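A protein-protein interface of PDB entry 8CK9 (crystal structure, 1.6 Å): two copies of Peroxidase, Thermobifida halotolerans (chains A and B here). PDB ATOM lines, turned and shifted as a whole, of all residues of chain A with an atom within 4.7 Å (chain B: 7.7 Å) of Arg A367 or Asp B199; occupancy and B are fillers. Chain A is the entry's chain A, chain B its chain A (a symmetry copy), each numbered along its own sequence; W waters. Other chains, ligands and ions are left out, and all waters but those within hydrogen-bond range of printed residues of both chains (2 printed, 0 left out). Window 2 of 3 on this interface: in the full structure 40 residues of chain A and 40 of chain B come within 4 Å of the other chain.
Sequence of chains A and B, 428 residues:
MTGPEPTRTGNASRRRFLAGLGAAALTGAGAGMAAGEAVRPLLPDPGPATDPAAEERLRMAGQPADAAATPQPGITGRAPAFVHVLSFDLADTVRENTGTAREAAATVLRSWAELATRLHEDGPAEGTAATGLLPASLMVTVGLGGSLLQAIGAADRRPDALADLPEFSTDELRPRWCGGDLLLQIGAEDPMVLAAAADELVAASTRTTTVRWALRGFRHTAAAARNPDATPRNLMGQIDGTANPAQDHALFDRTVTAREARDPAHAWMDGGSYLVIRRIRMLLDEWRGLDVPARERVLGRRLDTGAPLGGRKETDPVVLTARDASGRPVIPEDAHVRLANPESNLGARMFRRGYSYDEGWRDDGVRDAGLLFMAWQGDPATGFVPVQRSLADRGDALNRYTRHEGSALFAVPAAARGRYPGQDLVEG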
ATOM      1  N   ARG A 281     -17.479 -29.657  18.406  1.00  0.00           N
ATOM      2  CA  ARG A 281     -16.651 -28.571  18.905  1.00  0.00           C
ATOM      3  C   ARG A 281     -16.363 -27.600  17.769  1.00  0.00           C
ATOM      4  O   ARG A 281     -16.079 -28.011  16.644  1.00  0.00           O
ATOM      5  CB  ARG A 281     -15.356 -29.129  19.486  1.00  0.00           C
ATOM      6  CG  ARG A 281     -14.447 -28.069  20.066  1.00  0.00           C
ATOM      7  CD  ARG A 281     -13.326 -28.700  20.896  1.00  0.00           C
ATOM      8  NE  ARG A 281     -12.494 -29.607  20.114  1.00  0.00           N
ATOM      9  CZ  ARG A 281     -11.422 -29.236  19.426  1.00  0.00           C
ATOM     10  NH1 ARG A 281     -11.048 -27.970  19.361  1.00  0.00           N
ATOM     11  NH2 ARG A 281     -10.714 -30.157  18.779  1.00  0.00           N
ATOM     12  N   LEU A 284     -13.074 -21.974  17.482  1.00  0.00           N
ATOM     13  CA  LEU A 284     -13.415 -20.552  17.495  1.00  0.00           C
ATOM     14  C   LEU A 284     -12.189 -19.651  17.382  1.00  0.00           C
ATOM     15  O   LEU A 284     -12.296 -18.537  16.858  1.00  0.00           O
ATOM     16  CB  LEU A 284     -14.217 -20.217  18.756  1.00  0.00           C
ATOM     17  CG  LEU A 284     -15.613 -20.844  18.811  1.00  0.00           C
ATOM     18  CD1 LEU A 284     -16.251 -20.569  20.156  1.00  0.00           C
ATOM     19  CD2 LEU A 284     -16.477 -20.306  17.679  1.00  0.00           C
ATOM     20  N   ARG A 288     -11.971 -16.926  14.449  1.00  0.00           N
ATOM     21  CA  ARG A 288     -11.732 -15.514  14.716  1.00  0.00           C
ATOM     22  C   ARG A 288     -10.733 -14.909  13.738  1.00  0.00           C
ATOM     23  O   ARG A 288     -10.775 -13.699  13.494  1.00  0.00           O
ATOM     24  CB  ARG A 288     -11.254 -15.359  16.168  1.00  0.00           C
ATOM     25  CG  ARG A 288     -10.861 -13.961  16.588  1.00  0.00           C
ATOM     26  CD  ARG A 288     -10.717 -13.873  18.108  1.00  0.00           C
ATOM     27  NE  ARG A 288     -12.012 -13.769  18.772  1.00  0.00           N
ATOM     28  CZ  ARG A 288     -12.647 -12.625  18.985  1.00  0.00           C
ATOM     29  NH1 ARG A 288     -12.135 -11.469  18.598  1.00  0.00           N
ATOM     30  NH2 ARG A 288     -13.826 -12.641  19.601  1.00  0.00           N
ATOM     31  N   ASP A 358     -20.799 -24.742  26.151  1.00  0.00           N
ATOM     32  CA  ASP A 358     -19.515 -24.180  26.565  1.00  0.00           C
ATOM     33  C   ASP A 358     -19.026 -24.964  27.777  1.00  0.00           C
ATOM     34  O   ASP A 358     -19.561 -24.804  28.880  1.00  0.00           O
ATOM     35  CB  ASP A 358     -19.639 -22.690  26.891  1.00  0.00           C
ATOM     36  CG  ASP A 358     -18.287 -22.039  27.145  1.00  0.00           C
ATOM     37  OD1 ASP A 358     -17.273 -22.775  27.248  1.00  0.00           O
ATOM     38  OD2 ASP A 358     -18.240 -20.795  27.222  1.00  0.00           O
ATOM     39  N   GLY A 360     -15.808 -24.875  28.835  1.00  0.00           N
ATOM     40  CA  GLY A 360     -14.588 -24.266  29.363  1.00  0.00           C
ATOM     41  C   GLY A 360     -13.373 -24.619  28.543  1.00  0.00           C
ATOM     42  O   GLY A 360     -13.390 -24.539  27.313  1.00  0.00           O
ATOM     43  N   TRP A 361     -12.298 -24.992  29.228  1.00  0.00           N
ATOM     44  CA  TRP A 361     -11.025 -25.305  28.599  1.00  0.00           C
ATOM     45  C   TRP A 361     -10.606 -26.703  29.015  1.00  0.00           C
ATOM     46  O   TRP A 361     -10.689 -27.050  30.196  1.00  0.00           O
ATOM     47  CB  TRP A 361      -9.944 -24.285  28.990  1.00  0.00           C
ATOM     48  CG  TRP A 361     -10.096 -22.966  28.297  1.00  0.00           C
ATOM     49  CD1 TRP A 361      -9.444 -22.555  27.166  1.00  0.00           C
ATOM     50  CD2 TRP A 361     -10.970 -21.892  28.666  1.00  0.00           C
ATOM     51  NE1 TRP A 361      -9.858 -21.294  26.813  1.00  0.00           N
ATOM     52  CE2 TRP A 361     -10.797 -20.866  27.716  1.00  0.00           C
ATOM     53  CE3 TRP A 361     -11.886 -21.702  29.705  1.00  0.00           C
ATOM     54  CZ2 TRP A 361     -11.502 -19.666  27.774  1.00  0.00           C
ATOM     55  CZ3 TRP A 361     -12.594 -20.512  29.757  1.00  0.00           C
ATOM     56  CH2 TRP A 361     -12.392 -19.505  28.799  1.00  0.00           C
ATOM     57  N   GLY A 365      -5.530 -26.824  26.952  1.00  0.00           N
ATOM     58  CA  GLY A 365      -5.681 -25.388  26.854  1.00  0.00           C
ATOM     59  C   GLY A 365      -6.599 -24.887  25.760  1.00  0.00           C
ATOM     60  O   GLY A 365      -6.773 -23.669  25.637  1.00  0.00           O
ATOM     61  N   VAL A 366      -7.180 -25.765  24.959  1.00  0.00           N
ATOM     62  CA  VAL A 366      -8.071 -25.344  23.883  1.00  0.00           C
ATOM     63  C   VAL A 366      -9.492 -25.252  24.422  1.00  0.00           C
ATOM     64  O   VAL A 366      -9.923 -26.074  25.243  1.00  0.00           O
ATOM     65  CB  VAL A 366      -7.982 -26.304  22.681  1.00  0.00           C
ATOM     66  CG1 VAL A 366      -8.144 -27.721  23.144  1.00  0.00           C
ATOM     67  CG2 VAL A 366      -9.040 -25.968  21.622  1.00  0.00           C
ATOM     68  N   ARG A 367     -10.208 -24.229  23.972  1.00  0.00           N
ATOM     69  CA  ARG A 367     -11.592 -24.030  24.371  1.00  0.00           C
ATOM     70  C   ARG A 367     -12.449 -25.199  23.905  1.00  0.00           C
ATOM     71  O   ARG A 367     -12.329 -25.659  22.765  1.00  0.00           O
ATOM     72  CB  ARG A 367     -12.111 -22.716  23.784  1.00  0.00           C
ATOM     73  CG  ARG A 367     -13.538 -22.385  24.143  1.00  0.00           C
ATOM     74  CD  ARG A 367     -13.629 -21.069  24.894  1.00  0.00           C
ATOM     75  NE  ARG A 367     -15.014 -20.645  25.043  1.00  0.00           N
ATOM     76  CZ  ARG A 367     -15.652 -19.864  24.183  1.00  0.00           C
ATOM     77  NH1 ARG A 367     -15.045 -19.367  23.115  1.00  0.00           N
ATOM     78  NH2 ARG A 367     -16.933 -19.573  24.396  1.00  0.00           N
ATOM     79  N   ASP A 368     -13.309 -25.691  24.792  1.00  0.00           N
ATOM     80  CA  ASP A 368     -14.257 -26.747  24.442  1.00  0.00           C
ATOM     81  C   ASP A 368     -15.652 -26.130  24.447  1.00  0.00           C
ATOM     82  O   ASP A 368     -16.370 -26.173  25.448  1.00  0.00           O
ATOM     83  CB  ASP A 368     -14.170 -27.940  25.395  1.00  0.00           C
ATOM     84  CG  ASP A 368     -14.880 -29.167  24.847  1.00  0.00           C
ATOM     85  OD1 ASP A 368     -15.500 -29.065  23.763  1.00  0.00           O
ATOM     86  OD2 ASP A 368     -14.820 -30.230  25.496  1.00  0.00           O
ATOM     87  N   ALA A 369     -16.028 -25.556  23.309  1.00  0.00           N
ATOM     88  CA  ALA A 369     -17.339 -24.965  23.104  1.00  0.00           C
ATOM     89  C   ALA A 369     -17.753 -25.276  21.676  1.00  0.00           C
ATOM     90  O   ALA A 369     -16.912 -25.534  20.814  1.00  0.00           O
ATOM     91  CB  ALA A 369     -17.318 -23.446  23.341  1.00  0.00           C
ATOM     92  N   HIS B  84     -19.643 -15.290  34.486  1.00  0.00           N
ATOM     93  CA  HIS B  84     -18.496 -16.082  34.081  1.00  0.00           C
ATOM     94  C   HIS B  84     -17.316 -15.510  34.841  1.00  0.00           C
ATOM     95  O   HIS B  84     -16.990 -14.331  34.677  1.00  0.00           O
ATOM     96  CB  HIS B  84     -18.275 -16.025  32.565  1.00  0.00           C
ATOM     97  CG  HIS B  84     -17.487 -17.172  32.029  1.00  0.00           C
ATOM     98  ND1 HIS B  84     -17.505 -17.522  30.695  1.00  0.00           N
ATOM     99  CD2 HIS B  84     -16.659 -18.052  32.641  1.00  0.00           C
ATOM    100  CE1 HIS B  84     -16.713 -18.565  30.507  1.00  0.00           C
ATOM    101  NE2 HIS B  84     -16.186 -18.905  31.669  1.00  0.00           N
ATOM    102  N   LEU B  86     -13.369 -15.752  35.471  1.00  0.00           N
ATOM    103  CA  LEU B  86     -12.174 -16.261  34.808  1.00  0.00           C
ATOM    104  C   LEU B  86     -10.941 -15.778  35.542  1.00  0.00           C
ATOM    105  O   LEU B  86     -10.770 -14.573  35.754  1.00  0.00           O
ATOM    106  CB  LEU B  86     -12.105 -15.825  33.347  1.00  0.00           C
ATOM    107  CG  LEU B  86     -13.308 -16.232  32.500  1.00  0.00           C
ATOM    108  CD1 LEU B  86     -14.248 -15.065  32.321  1.00  0.00           C
ATOM    109  CD2 LEU B  86     -12.837 -16.760  31.165  1.00  0.00           C
ATOM    110  N   LEU B 115     -11.783  -2.554  25.920  1.00  0.00           N
ATOM    111  CA  LEU B 115     -12.851  -3.411  25.433  1.00  0.00           C
ATOM    112  C   LEU B 115     -14.061  -3.362  26.356  1.00  0.00           C
ATOM    113  O   LEU B 115     -15.200  -3.312  25.884  1.00  0.00           O
ATOM    114  CB  LEU B 115     -12.324  -4.836  25.285  1.00  0.00           C
ATOM    115  CG  LEU B 115     -13.307  -5.906  24.821  1.00  0.00           C
ATOM    116  CD1 LEU B 115     -13.960  -5.512  23.503  1.00  0.00           C
ATOM    117  CD2 LEU B 115     -12.566  -7.222  24.677  1.00  0.00           C
ATOM    118  N   GLY B 127     -21.664  -9.272  14.284  1.00  0.00           N
ATOM    119  CA  GLY B 127     -20.899 -10.437  13.900  1.00  0.00           C
ATOM    120  C   GLY B 127     -20.485 -11.336  15.040  1.00  0.00           C
ATOM    121  O   GLY B 127     -19.657 -12.231  14.835  1.00  0.00           O
ATOM    122  N   THR B 128     -21.015 -11.125  16.240  1.00  0.00           N
ATOM    123  CA  THR B 128     -20.790 -12.041  17.346  1.00  0.00           C
ATOM    124  C   THR B 128     -22.058 -12.845  17.610  1.00  0.00           C
ATOM    125  O   THR B 128     -23.095 -12.653  16.963  1.00  0.00           O
ATOM    126  CB  THR B 128     -20.363 -11.293  18.612  1.00  0.00           C
ATOM    127  OG1 THR B 128     -21.469 -10.523  19.107  1.00  0.00           O
ATOM    128  CG2 THR B 128     -19.181 -10.369  18.313  1.00  0.00           C
ATOM    129  N   ALA B 129     -21.962 -13.754  18.586  1.00  0.00           N
ATOM    130  CA  ALA B 129     -23.117 -14.539  18.999  1.00  0.00           C
ATOM    131  C   ALA B 129     -24.241 -13.671  19.546  1.00  0.00           C
ATOM    132  O   ALA B 129     -25.393 -14.119  19.580  1.00  0.00           O
ATOM    133  CB  ALA B 129     -22.697 -15.570  20.050  1.00  0.00           C
ATOM    134  N   ILE B 186     -17.469 -11.448  34.563  1.00  0.00           N
ATOM    135  CA  ILE B 186     -18.337 -10.973  33.495  1.00  0.00           C
ATOM    136  C   ILE B 186     -19.753 -11.393  33.837  1.00  0.00           C
ATOM    137  O   ILE B 186     -19.996 -12.567  34.137  1.00  0.00           O
ATOM    138  CB  ILE B 186     -17.919 -11.538  32.126  1.00  0.00           C
ATOM    139  CG1 ILE B 186     -16.399 -11.435  31.927  1.00  0.00           C
ATOM    140  CG2 ILE B 186     -18.673 -10.826  31.017  1.00  0.00           C
ATOM    141  CD1 ILE B 186     -15.914 -12.152  30.689  1.00  0.00           C
ATOM    142  N   VAL B 193     -25.230 -13.102  25.288  1.00  0.00           N
ATOM    143  CA  VAL B 193     -24.513 -11.851  25.515  1.00  0.00           C
ATOM    144  C   VAL B 193     -23.249 -12.119  26.318  1.00  0.00           C
ATOM    145  O   VAL B 193     -22.157 -11.633  25.984  1.00  0.00           O
ATOM    146  CB  VAL B 193     -25.435 -10.838  26.214  1.00  0.00           C
ATOM    147  CG1 VAL B 193     -24.641  -9.599  26.636  1.00  0.00           C
ATOM    148  CG2 VAL B 193     -26.571 -10.452  25.282  1.00  0.00           C
ATOM    149  N   LEU B 194     -23.369 -12.942  27.362  1.00  0.00           N
ATOM    150  CA  LEU B 194     -22.219 -13.291  28.189  1.00  0.00           C
ATOM    151  C   LEU B 194     -21.158 -14.019  27.375  1.00  0.00           C
ATOM    152  O   LEU B 194     -19.968 -13.688  27.445  1.00  0.00           O
ATOM    153  CB  LEU B 194     -22.692 -14.150  29.361  1.00  0.00           C
ATOM    154  CG  LEU B 194     -21.566 -14.583  30.297  1.00  0.00           C
ATOM    155  CD1 LEU B 194     -21.026 -13.368  30.998  1.00  0.00           C
ATOM    156  CD2 LEU B 194     -22.047 -15.628  31.299  1.00  0.00           C
ATOM    157  N   ALA B 195     -21.576 -15.013  26.588  1.00  0.00           N
ATOM    158  CA  ALA B 195     -20.618 -15.807  25.825  1.00  0.00           C
ATOM    159  C   ALA B 195     -19.868 -14.939  24.826  1.00  0.00           C
ATOM    160  O   ALA B 195     -18.660 -15.106  24.633  1.00  0.00           O
ATOM    161  CB  ALA B 195     -21.339 -16.952  25.107  1.00  0.00           C
ATOM    162  N   ALA B 196     -20.571 -14.003  24.179  1.00  0.00           N
ATOM    163  CA  ALA B 196     -19.908 -13.156  23.195  1.00  0.00           C
ATOM    164  C   ALA B 196     -18.900 -12.226  23.858  1.00  0.00           C
ATOM    165  O   ALA B 196     -17.795 -12.036  23.343  1.00  0.00           O
ATOM    166  CB  ALA B 196     -20.946 -12.361  22.405  1.00  0.00           C
ATOM    167  N   ALA B 197     -19.256 -11.650  25.010  1.00  0.00           N
ATOM    168  CA  ALA B 197     -18.331 -10.756  25.707  1.00  0.00           C
ATOM    169  C   ALA B 197     -17.119 -11.517  26.224  1.00  0.00           C
ATOM    170  O   ALA B 197     -15.984 -11.045  26.093  1.00  0.00           O
ATOM    171  CB  ALA B 197     -19.056 -10.050  26.854  1.00  0.00           C
ATOM    172  N   ALA B 198     -17.341 -12.705  26.802  1.00  0.00           N
ATOM    173  CA  ALA B 198     -16.231 -13.500  27.311  1.00  0.00           C
ATOM    174  C   ALA B 198     -15.270 -13.877  26.189  1.00  0.00           C
ATOM    175  O   ALA B 198     -14.048 -13.831  26.376  1.00  0.00           O
ATOM    176  CB  ALA B 198     -16.751 -14.751  28.024  1.00  0.00           C
ATOM    177  N   ASP B 199     -15.801 -14.233  25.013  1.00  0.00           N
ATOM    178  CA  ASP B 199     -14.937 -14.592  23.888  1.00  0.00           C
ATOM    179  C   ASP B 199     -14.045 -13.424  23.487  1.00  0.00           C
ATOM    180  O   ASP B 199     -12.843 -13.601  23.241  1.00  0.00           O
ATOM    181  CB  ASP B 199     -15.782 -15.056  22.700  1.00  0.00           C
ATOM    182  CG  ASP B 199     -14.945 -15.313  21.457  1.00  0.00           C
ATOM    183  OD1 ASP B 199     -14.181 -16.304  21.455  1.00  0.00           O
ATOM    184  OD2 ASP B 199     -15.045 -14.532  20.482  1.00  0.00           O
ATOM    185  N   GLU B 200     -14.622 -12.221  23.399  1.00  0.00           N
ATOM    186  CA  GLU B 200     -13.832 -11.051  23.024  1.00  0.00           C
ATOM    187  C   GLU B 200     -12.778 -10.743  24.073  1.00  0.00           C
ATOM    188  O   GLU B 200     -11.644 -10.376  23.739  1.00  0.00           O
ATOM    189  CB  GLU B 200     -14.731  -9.834  22.835  1.00  0.00           C
ATOM    190  CG  GLU B 200     -15.775  -9.971  21.748  1.00  0.00           C
ATOM    191  CD  GLU B 200     -16.465  -8.654  21.453  1.00  0.00           C
ATOM    192  OE1 GLU B 200     -15.775  -7.611  21.464  1.00  0.00           O
ATOM    193  OE2 GLU B 200     -17.693  -8.660  21.219  1.00  0.00           O
ATOM    194  N   LEU B 201     -13.135 -10.865  25.354  1.00  0.00           N
ATOM    195  CA  LEU B 201     -12.188 -10.491  26.398  1.00  0.00           C
ATOM    196  C   LEU B 201     -11.044 -11.495  26.491  1.00  0.00           C
ATOM    197  O   LEU B 201      -9.887 -11.111  26.696  1.00  0.00           O
ATOM    198  CB  LEU B 201     -12.923 -10.358  27.730  1.00  0.00           C
ATOM    199  CG  LEU B 201     -13.763  -9.085  27.857  1.00  0.00           C
ATOM    200  CD1 LEU B 201     -14.832  -9.257  28.920  1.00  0.00           C
ATOM    201  CD2 LEU B 201     -12.861  -7.884  28.189  1.00  0.00           C
ATOM    202  N   VAL B 202     -11.344 -12.787  26.334  1.00  0.00           N
ATOM    203  CA  VAL B 202     -10.282 -13.786  26.334  1.00  0.00           C
ATOM    204  C   VAL B 202      -9.387 -13.598  25.116  1.00  0.00           C
ATOM    205  O   VAL B 202      -8.161 -13.711  25.214  1.00  0.00           O
ATOM    206  CB  VAL B 202     -10.874 -15.206  26.397  1.00  0.00           C
ATOM    207  CG1 VAL B 202      -9.782 -16.254  26.137  1.00  0.00           C
ATOM    208  CG2 VAL B 202     -11.504 -15.460  27.750  1.00  0.00           C
ATOM    209  N   ALA B 203      -9.975 -13.283  23.956  1.00  0.00           N
ATOM    210  CA  ALA B 203      -9.160 -13.087  22.759  1.00  0.00           C
ATOM    211  C   ALA B 203      -8.164 -11.954  22.951  1.00  0.00           C
ATOM    212  O   ALA B 203      -7.038 -12.011  22.438  1.00  0.00           O
ATOM    213  CB  ALA B 203     -10.053 -12.808  21.548  1.00  0.00           C
ATOM    214  N   ALA B 204      -8.553 -10.924  23.703  1.00  0.00           N
ATOM    215  CA  ALA B 204      -7.688  -9.780  23.943  1.00  0.00           C
ATOM    216  C   ALA B 204      -6.522 -10.119  24.852  1.00  0.00           C
ATOM    217  O   ALA B 204      -5.592  -9.319  24.957  1.00  0.00           O
ATOM    218  CB  ALA B 204      -8.496  -8.633  24.548  1.00  0.00           C
ATOM    219  N   SER B 205      -6.551 -11.279  25.497  1.00  0.00           N
ATOM    220  CA  SER B 205      -5.571 -11.646  26.508  1.00  0.00           C
ATOM    221  C   SER B 205      -4.581 -12.701  26.028  1.00  0.00           C
ATOM    222  O   SER B 205      -3.704 -13.098  26.800  1.00  0.00           O
ATOM    223  CB  SER B 205      -6.306 -12.150  27.759  1.00  0.00           C
ATOM    224  OG  SER B 205      -6.760 -13.485  27.564  1.00  0.00           O
ATOM    225  N   THR B 206      -4.680 -13.153  24.772  1.00  0.00           N
ATOM    226  CA  THR B 206      -4.028 -14.409  24.391  1.00  0.00           C
ATOM    227  C   THR B 206      -2.507 -14.311  24.398  1.00  0.00           C
ATOM    228  O   THR B 206      -1.826 -15.289  24.730  1.00  0.00           O
ATOM    229  CB  THR B 206      -4.509 -14.874  23.016  1.00  0.00           C
ATOM    230  OG1 THR B 206      -4.256 -13.854  22.041  1.00  0.00           O
ATOM    231  CG2 THR B 206      -5.991 -15.195  23.061  1.00  0.00           C
ATOM    232  N   ARG B 216     -18.540 -20.891  35.095  1.00  0.00           N
ATOM    233  CA  ARG B 216     -19.778 -20.216  34.766  1.00  0.00           C
ATOM    234  C   ARG B 216     -20.793 -20.488  35.869  1.00  0.00           C
ATOM    235  O   ARG B 216     -20.855 -21.600  36.411  1.00  0.00           O
ATOM    236  CB  ARG B 216     -20.315 -20.693  33.412  1.00  0.00           C
ATOM    237  CG  ARG B 216     -19.389 -20.343  32.243  1.00  0.00           C
ATOM    238  CD  ARG B 216     -19.766 -21.047  30.949  1.00  0.00           C
ATOM    239  NE  ARG B 216     -21.007 -20.542  30.378  1.00  0.00           N
ATOM    240  CZ  ARG B 216     -22.114 -21.258  30.230  1.00  0.00           C
ATOM    241  NH1 ARG B 216     -22.166 -22.529  30.590  1.00  0.00           N
ATOM    242  NH2 ARG B 216     -23.192 -20.684  29.700  1.00  0.00           N
HETATM  243  O   HOH W   1     -18.136 -17.726  22.848  1.00  0.00           O
HETATM  244  O   HOH W   2     -12.057 -16.398  19.664  1.00  0.00           O
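The guanidinium group (NH2) of Arg A288 is in salt-bridge range of the side-chain carboxylate (OD2) of Asp B199.
NH1 of Arg A367 is in salt-bridge range of OD1 of Asp B199, at 3.6 Å.
No position is printed for both chains.
Of the 11 printed residues of chain A, 4 touch a printed residue of chain B.
Printed residues of chain A that touch a printed residue of chain B: Arg A288, Asp A358, Trp A361 and Arg A367.
Hydrophobic or aromatic side chains of chain A within 4 Å of the printed part of chain B: Trp A361.
Of the 22 printed residues of chain B, 5 touch a printed residue of chain A.
Hydrophobic or aromatic side chains of chain B within 4 Å of the printed part of chain A: Leu B86 and Ala B203.
Among the printed residues, Asp or Glu carboxylates within 4 Å of a Lys or Arg side-chain nitrogen of the other chain: Arg A288 with Asp B199 and Arg A367 with Asp B199.
Glu B200 touches Arg A288.
Arg A288 touches Ala B203.
Asp A358 touches Arg B216 (O to NH1, 3.9 Å).
Leu B86 touches Trp A361.
OG1 of Thr B206 is in hydrogen-bond range of O of Ala B203 (3.4 Å).
OD1 of Asp A358 sits at hydrogen-bond distance from N of Gly A360.
The side-chain carboxylate of Asp A358 lies within salt-bridge range of the guanidinium group of Arg A367.
Of chain A, only Arg A288 (2.4 Å) and Arg A367 (3.6 Å) come within 4 Å of Asp B199.
Of the printed residues of chain B, Asp A358 touches Arg B216.
Of the printed residues of chain A, Glu B200 touches Arg A288 (3.8 Å).
Printed residues of chain B within 4 Å of Arg A288: Asp B199 (2.4 Å), Glu B200 (3.8 Å) and Ala B203 (3.5 Å).
Ala B198 touches none of the printed residues of chain A.
Val A366 touches none of the printed residues of chain B.
The nearest printed residue of chain A that does not touch Asp B199 is Leu A284 (4.8 Å).
The nearest printed residue of chain A that does not touch Ala B203 is Trp A361 (7.6 Å).
Water W1 lies within hydrogen-bond range of the guanidinium group (NH2) of Arg A367 and the backbone carbonyl oxygen (O) of Ala B195.
Water W2 bridges NE of Arg A288 (2.8 Å) and OD1 of Asp B199 (2.8 Å).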
